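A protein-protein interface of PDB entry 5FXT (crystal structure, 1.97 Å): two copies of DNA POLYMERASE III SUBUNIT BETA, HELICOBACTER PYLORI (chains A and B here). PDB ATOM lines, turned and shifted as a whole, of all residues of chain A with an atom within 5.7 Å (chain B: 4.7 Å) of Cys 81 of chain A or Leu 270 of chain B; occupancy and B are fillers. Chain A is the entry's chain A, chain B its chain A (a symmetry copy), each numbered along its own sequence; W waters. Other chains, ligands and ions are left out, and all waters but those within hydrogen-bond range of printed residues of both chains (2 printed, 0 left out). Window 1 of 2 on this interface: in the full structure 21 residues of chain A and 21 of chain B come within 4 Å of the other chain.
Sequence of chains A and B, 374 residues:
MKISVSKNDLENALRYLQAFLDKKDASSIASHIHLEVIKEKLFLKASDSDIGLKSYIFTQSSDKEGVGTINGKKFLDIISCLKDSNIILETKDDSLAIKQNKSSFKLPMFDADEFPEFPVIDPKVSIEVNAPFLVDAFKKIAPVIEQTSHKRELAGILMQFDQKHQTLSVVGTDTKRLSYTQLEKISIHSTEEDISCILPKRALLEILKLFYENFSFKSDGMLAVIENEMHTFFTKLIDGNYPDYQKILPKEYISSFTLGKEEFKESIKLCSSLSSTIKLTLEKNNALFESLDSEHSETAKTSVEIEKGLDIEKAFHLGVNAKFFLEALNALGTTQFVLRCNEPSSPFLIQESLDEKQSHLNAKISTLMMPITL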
ATOM      1  N   LYS A   7      16.019 -15.439  10.992  1.00  0.00           N
ATOM      2  CA  LYS A   7      14.828 -15.995  10.348  1.00  0.00           C
ATOM      3  C   LYS A   7      14.449 -17.328  10.901  1.00  0.00           C
ATOM      4  O   LYS A   7      13.310 -17.538  11.276  1.00  0.00           O
ATOM      5  CB  LYS A   7      15.016 -16.040   8.819  1.00  0.00           C
ATOM      6  CG  LYS A   7      13.794 -16.517   8.005  1.00  0.00           C
ATOM      7  CD  LYS A   7      13.649 -18.034   7.971  1.00  0.00           C
ATOM      8  CE  LYS A   7      13.000 -18.496   6.681  1.00  0.00           C
ATOM      9  NZ  LYS A   7      12.748 -19.944   6.796  1.00  0.00           N
ATOM     10  N   LEU A  76       3.640 -16.108  11.047  1.00  0.00           N
ATOM     11  CA  LEU A  76       4.336 -17.323  10.683  1.00  0.00           C
ATOM     12  C   LEU A  76       4.264 -17.515   9.128  1.00  0.00           C
ATOM     13  O   LEU A  76       5.272 -17.884   8.536  1.00  0.00           O
ATOM     14  CB  LEU A  76       3.814 -18.527  11.439  1.00  0.00           C
ATOM     15  CG  LEU A  76       4.327 -19.918  10.949  1.00  0.00           C
ATOM     16  CD1 LEU A  76       5.838 -20.199  11.097  1.00  0.00           C
ATOM     17  CD2 LEU A  76       3.546 -21.033  11.579  1.00  0.00           C
ATOM     18  N   ASP A  77       3.150 -17.159   8.485  1.00  0.00           N
ATOM     19  CA  ASP A  77       3.023 -17.447   7.031  1.00  0.00           C
ATOM     20  C   ASP A  77       4.015 -16.574   6.290  1.00  0.00           C
ATOM     21  O   ASP A  77       4.708 -17.073   5.432  1.00  0.00           O
ATOM     22  CB  ASP A  77       1.641 -17.221   6.514  1.00  0.00           C
ATOM     23  CG  ASP A  77       0.634 -18.305   6.943  1.00  0.00           C
ATOM     24  OD1 ASP A  77       1.012 -19.379   7.407  1.00  0.00           O
ATOM     25  OD2 ASP A  77      -0.562 -18.011   6.865  1.00  0.00           O
ATOM     26  N   ILE A  78       4.180 -15.313   6.711  1.00  0.00           N
ATOM     27  CA  ILE A  78       5.172 -14.432   6.070  1.00  0.00           C
ATOM     28  C   ILE A  78       6.620 -14.863   6.202  1.00  0.00           C
ATOM     29  O   ILE A  78       7.384 -14.798   5.224  1.00  0.00           O
ATOM     30  CB  ILE A  78       5.044 -12.987   6.605  1.00  0.00           C
ATOM     31  CG1 ILE A  78       3.744 -12.402   6.095  1.00  0.00           C
ATOM     32  CG2 ILE A  78       6.230 -12.121   6.161  1.00  0.00           C
ATOM     33  CD1 ILE A  78       3.278 -11.212   6.903  1.00  0.00           C
ATOM     34  N   ILE A  79       6.998 -15.241   7.407  1.00  0.00           N
ATOM     35  CA  ILE A  79       8.355 -15.567   7.732  1.00  0.00           C
ATOM     36  C   ILE A  79       8.771 -16.891   7.107  1.00  0.00           C
ATOM     37  O   ILE A  79       9.946 -17.042   6.749  1.00  0.00           O
ATOM     38  CB  ILE A  79       8.564 -15.720   9.268  1.00  0.00           C
ATOM     39  CG1 ILE A  79       8.270 -14.374   9.982  1.00  0.00           C
ATOM     40  CG2 ILE A  79       9.984 -16.152   9.599  1.00  0.00           C
ATOM     41  CD1 ILE A  79       9.188 -13.251   9.617  1.00  0.00           C
ATOM     42  N   SER A  80       7.831 -17.853   7.008  1.00  0.00           N
ATOM     43  CA  SER A  80       8.141 -19.081   6.313  1.00  0.00           C
ATOM     44  C   SER A  80       8.434 -18.879   4.811  1.00  0.00           C
ATOM     45  O   SER A  80       9.034 -19.752   4.216  1.00  0.00           O
ATOM     46  CB  SER A  80       7.081 -20.165   6.579  1.00  0.00           C
ATOM     47  OG  SER A  80       5.881 -19.677   6.050  1.00  0.00           O
ATOM     48  N   CYS A  81       8.015 -17.768   4.220  1.00  0.00           N
ATOM     49  CA  CYS A  81       8.266 -17.474   2.789  1.00  0.00           C
ATOM     50  C   CYS A  81       9.559 -16.632   2.475  1.00  0.00           C
ATOM     51  O   CYS A  81       9.821 -16.305   1.302  1.00  0.00           O
ATOM     52  CB  CYS A  81       6.996 -16.810   2.165  1.00  0.00           C
ATOM     53  SG  CYS A  81       5.750 -18.056   1.700  1.00  0.00           S
ATOM     54  N   LEU A  82      10.338 -16.312   3.503  1.00  0.00           N
ATOM     55  CA  LEU A  82      11.571 -15.516   3.380  1.00  0.00           C
ATOM     56  C   LEU A  82      12.841 -16.378   3.417  1.00  0.00           C
ATOM     57  O   LEU A  82      12.808 -17.558   3.802  1.00  0.00           O
ATOM     58  CB  LEU A  82      11.629 -14.471   4.507  1.00  0.00           C
ATOM     59  CG  LEU A  82      10.521 -13.425   4.359  1.00  0.00           C
ATOM     60  CD1 LEU A  82      10.434 -12.618   5.671  1.00  0.00           C
ATOM     61  CD2 LEU A  82      10.741 -12.526   3.152  1.00  0.00           C
ATOM     62  N   LYS A  83      13.960 -15.750   3.031  1.00  0.00           N
ATOM     63  CA  LYS A  83      15.275 -16.417   2.928  1.00  0.00           C
ATOM     64  C   LYS A  83      15.913 -16.539   4.297  1.00  0.00           C
ATOM     65  O   LYS A  83      15.390 -15.973   5.252  1.00  0.00           O
ATOM     66  CB  LYS A  83      16.156 -15.688   1.915  1.00  0.00           C
ATOM     67  CG  LYS A  83      15.555 -15.670   0.497  1.00  0.00           C
ATOM     68  CD  LYS A  83      14.844 -14.368   0.119  1.00  0.00           C
ATOM     69  CE  LYS A  83      13.367 -14.567  -0.262  1.00  0.00           C
ATOM     70  NZ  LYS A  83      13.095 -15.432  -1.458  1.00  0.00           N
ATOM     71  N   SER A 103      12.088  -7.503   0.258  1.00  0.00           N
ATOM     72  CA  SER A 103      10.749  -7.927   0.667  1.00  0.00           C
ATOM     73  C   SER A 103      10.349  -7.145   1.912  1.00  0.00           C
ATOM     74  O   SER A 103      11.123  -7.135   2.903  1.00  0.00           O
ATOM     75  CB  SER A 103      10.771  -9.419   0.936  1.00  0.00           C
ATOM     76  OG  SER A 103      10.983 -10.177  -0.273  1.00  0.00           O
ATOM     77  N   PHE A 105       6.731  -6.171   4.556  1.00  0.00           N
ATOM     78  CA  PHE A 105       5.347  -6.417   5.001  1.00  0.00           C
ATOM     79  C   PHE A 105       4.935  -5.485   6.135  1.00  0.00           C
ATOM     80  O   PHE A 105       5.790  -5.032   6.925  1.00  0.00           O
ATOM     81  CB  PHE A 105       5.176  -7.832   5.475  1.00  0.00           C
ATOM     82  CG  PHE A 105       5.862  -8.857   4.626  1.00  0.00           C
ATOM     83  CD1 PHE A 105       7.225  -9.103   4.784  1.00  0.00           C
ATOM     84  CD2 PHE A 105       5.152  -9.564   3.657  1.00  0.00           C
ATOM     85  CE1 PHE A 105       7.870  -9.997   3.977  1.00  0.00           C
ATOM     86  CE2 PHE A 105       5.789 -10.511   2.859  1.00  0.00           C
ATOM     87  CZ  PHE A 105       7.158 -10.733   3.020  1.00  0.00           C
ATOM     88  N   GLU B 266       8.597 -17.723  -6.283  1.00  0.00           N
ATOM     89  CA  GLU B 266       8.945 -17.288  -4.862  1.00  0.00           C
ATOM     90  C   GLU B 266       8.286 -15.958  -4.553  1.00  0.00           C
ATOM     91  O   GLU B 266       7.817 -15.739  -3.488  1.00  0.00           O
ATOM     92  CB  GLU B 266      10.424 -17.112  -4.703  1.00  0.00           C
ATOM     93  CG  GLU B 266      11.130 -18.391  -5.008  1.00  0.00           C
ATOM     94  CD  GLU B 266      12.643 -18.300  -4.884  1.00  0.00           C
ATOM     95  OE1 GLU B 266      13.257 -17.209  -5.110  1.00  0.00           O
ATOM     96  OE2 GLU B 266      13.202 -19.393  -4.610  1.00  0.00           O
ATOM     97  N   SER B 267       8.334 -14.985  -5.494  1.00  0.00           N
ATOM     98  CA  SER B 267       7.710 -13.683  -5.256  1.00  0.00           C
ATOM     99  C   SER B 267       6.180 -13.703  -5.099  1.00  0.00           C
ATOM    100  O   SER B 267       5.606 -13.054  -4.195  1.00  0.00           O
ATOM    101  CB  SER B 267       8.166 -12.642  -6.327  1.00  0.00           C
ATOM    102  OG  SER B 267       9.608 -12.749  -6.374  1.00  0.00           O
ATOM    103  N   ILE B 268       5.537 -14.507  -5.905  1.00  0.00           N
ATOM    104  CA  ILE B 268       4.111 -14.669  -5.865  1.00  0.00           C
ATOM    105  C   ILE B 268       3.688 -15.417  -4.594  1.00  0.00           C
ATOM    106  O   ILE B 268       2.732 -15.016  -3.970  1.00  0.00           O
ATOM    107  CB  ILE B 268       3.598 -15.353  -7.146  1.00  0.00           C
ATOM    108  CG1 ILE B 268       3.754 -14.313  -8.277  1.00  0.00           C
ATOM    109  CG2 ILE B 268       2.168 -15.746  -6.974  1.00  0.00           C
ATOM    110  CD1 ILE B 268       3.618 -14.756  -9.724  1.00  0.00           C
ATOM    111  N   LYS B 269       4.367 -16.480  -4.290  1.00  0.00           N
ATOM    112  CA  LYS B 269       4.056 -17.254  -3.076  1.00  0.00           C
ATOM    113  C   LYS B 269       4.197 -16.318  -1.897  1.00  0.00           C
ATOM    114  O   LYS B 269       3.358 -16.312  -1.004  1.00  0.00           O
ATOM    115  CB  LYS B 269       5.034 -18.413  -2.870  1.00  0.00           C
ATOM    116  CG  LYS B 269       4.726 -19.606  -3.711  1.00  0.00           C
ATOM    117  CD  LYS B 269       5.798 -20.686  -3.642  1.00  0.00           C
ATOM    118  CE  LYS B 269       5.668 -21.575  -4.885  1.00  0.00           C
ATOM    119  NZ  LYS B 269       6.343 -22.918  -4.722  1.00  0.00           N
ATOM    120  N   LEU B 270       5.274 -15.538  -1.891  1.00  0.00           N
ATOM    121  CA  LEU B 270       5.548 -14.634  -0.737  1.00  0.00           C
ATOM    122  C   LEU B 270       4.383 -13.681  -0.554  1.00  0.00           C
ATOM    123  O   LEU B 270       3.869 -13.582   0.564  1.00  0.00           O
ATOM    124  CB  LEU B 270       6.884 -13.921  -0.914  1.00  0.00           C
ATOM    125  CG  LEU B 270       7.388 -12.820  -0.027  1.00  0.00           C
ATOM    126  CD1 LEU B 270       8.876 -12.603  -0.257  1.00  0.00           C
ATOM    127  CD2 LEU B 270       6.673 -11.504  -0.301  1.00  0.00           C
ATOM    128  N   CYS B 271       3.898 -13.025  -1.639  1.00  0.00           N
ATOM    129  CA  CYS B 271       2.803 -12.063  -1.530  1.00  0.00           C
ATOM    130  C   CYS B 271       1.484 -12.719  -1.241  1.00  0.00           C
ATOM    131  O   CYS B 271       0.632 -12.107  -0.596  1.00  0.00           O
ATOM    132  CB  CYS B 271       2.678 -11.161  -2.782  1.00  0.00           C
ATOM    133  SG  CYS B 271       4.073 -10.066  -2.967  1.00  0.00           S
ATOM    134  N   SER B 272       1.332 -13.970  -1.654  1.00  0.00           N
ATOM    135  CA  SER B 272       0.107 -14.687  -1.439  1.00  0.00           C
ATOM    136  C   SER B 272      -0.071 -15.109   0.076  1.00  0.00           C
ATOM    137  O   SER B 272      -1.143 -15.537   0.492  1.00  0.00           O
ATOM    138  CB  SER B 272       0.021 -15.874  -2.392  1.00  0.00           C
ATOM    139  OG  SER B 272       0.789 -16.924  -1.921  1.00  0.00           O
ATOM    140  N   SER B 273       0.967 -14.987   0.890  1.00  0.00           N
ATOM    141  CA  SER B 273       0.787 -15.138   2.330  1.00  0.00           C
ATOM    142  C   SER B 273      -0.347 -14.250   2.890  1.00  0.00           C
ATOM    143  O   SER B 273      -0.982 -14.634   3.870  1.00  0.00           O
ATOM    144  CB  SER B 273       2.102 -14.934   3.063  1.00  0.00           C
ATOM    145  OG  SER B 273       2.551 -13.598   2.961  1.00  0.00           O
ATOM    146  N   ALA B 300       1.910  -7.021   1.660  1.00  0.00           N
ATOM    147  CA  ALA B 300       3.125  -7.756   1.306  1.00  0.00           C
ATOM    148  C   ALA B 300       3.709  -7.217  -0.011  1.00  0.00           C
ATOM    149  O   ALA B 300       2.993  -7.141  -0.968  1.00  0.00           O
ATOM    150  CB  ALA B 300       2.830  -9.228   1.200  1.00  0.00           C
ATOM    151  N   LYS B 301       4.991  -6.834  -0.042  1.00  0.00           N
ATOM    152  CA  LYS B 301       5.683  -6.386  -1.259  1.00  0.00           C
ATOM    153  C   LYS B 301       7.049  -7.058  -1.429  1.00  0.00           C
ATOM    154  O   LYS B 301       7.801  -7.327  -0.439  1.00  0.00           O
ATOM    155  CB  LYS B 301       5.896  -4.885  -1.267  1.00  0.00           C
ATOM    156  CG  LYS B 301       4.632  -4.081  -0.949  1.00  0.00           C
ATOM    157  CD  LYS B 301       4.917  -2.629  -0.628  1.00  0.00           C
ATOM    158  CE  LYS B 301       5.727  -1.926  -1.726  1.00  0.00           C
ATOM    159  NZ  LYS B 301       5.614  -0.434  -1.638  1.00  0.00           N
ATOM    160  N   THR B 302       7.374  -7.342  -2.699  1.00  0.00           N
ATOM    161  CA  THR B 302       8.702  -7.745  -3.020  1.00  0.00           C
ATOM    162  C   THR B 302       9.089  -7.319  -4.382  1.00  0.00           C
ATOM    163  O   THR B 302       8.239  -6.875  -5.125  1.00  0.00           O
ATOM    164  CB  THR B 302       8.977  -9.217  -2.742  1.00  0.00           C
ATOM    165  OG1 THR B 302      10.388  -9.407  -2.619  1.00  0.00           O
ATOM    166  CG2 THR B 302       8.391 -10.090  -3.767  1.00  0.00           C
HETATM  167  O   HOH W   1       8.377 -17.427  -1.515  1.00  0.00           O
HETATM  168  O   HOH W   2      -1.377 -15.606   6.306  1.00  0.00           O
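Of the printed residues of chain B, Cys 81 of chain A touches Leu 270.
Ser 267 of chain B touches none of the printed residues of chain A.
Of chain A, only Cys 81, Leu 82, Ser 103 and Phe 105 come within 4 Å of Leu 270 of chain B.
Of the printed residues of chain A, Ser 273 of chain B touches Ile 78 (3.6 Å).
Printed residues of chain A within 4 Å of Ala 300 of chain B: Phe 105 (3.4 Å).
Printed residues of chain A within 4 Å of Lys 301 of chain B: Ser 103.
The nearest printed residue of chain B that does not touch Cys 81 of chain A is Lys 269 of chain B (4.01 Å).
The nearest residue of chain A that does not touch Leu 270 of chain B is Lys 83 of chain A (4.9 Å).
Among the printed residues, merely in contact across the chains: Ile 78 of chain A with Ser 273 of chain B, Cys 81 of chain A with Leu 270 of chain B, Leu 82 of chain A with Leu 270 of chain B, Ser 103 of chain A with Leu 270 of chain B, Ser 103 of chain A with Lys 301 of chain B, Phe 105 of chain A with Leu 270 of chain B and Phe 105 of chain A with Ala 300 of chain B.
The side-chain hydroxyl (OG) of Ser 273 of chain B lies within hydrogen-bond range of the backbone carbonyl oxygen (O) of Leu 270 of chain B.
SG of Cys 271 of chain B sits at hydrogen-bond distance from O of Ala 300 of chain B (3.7 Å).
Hydrophobic or aromatic side chains of chain B within 4 Å of the printed part of chain A: Leu 270 and Ala 300.
Among the printed residues, 8 pairs touch across the chains.
No position is printed for both chains.
Of the 8 pairs that touch across the chains among the printed residues, none has its exchanged pair printed and touching as well.
The side-chain hydroxyl (OG) of Ser 103 of chain A sits at hydrogen-bond distance from the side-chain hydroxyl (OG1) of Thr 302 of chain B, at 2.5 Å.
Water W2 bridges OD2 of Asp 77 of chain A and O of Ser 273 of chain B.
Water W1 bridges the backbone carbonyl oxygen of Glu 266 of chain B and the backbone carbonyl oxygen of Cys 81 of chain A.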
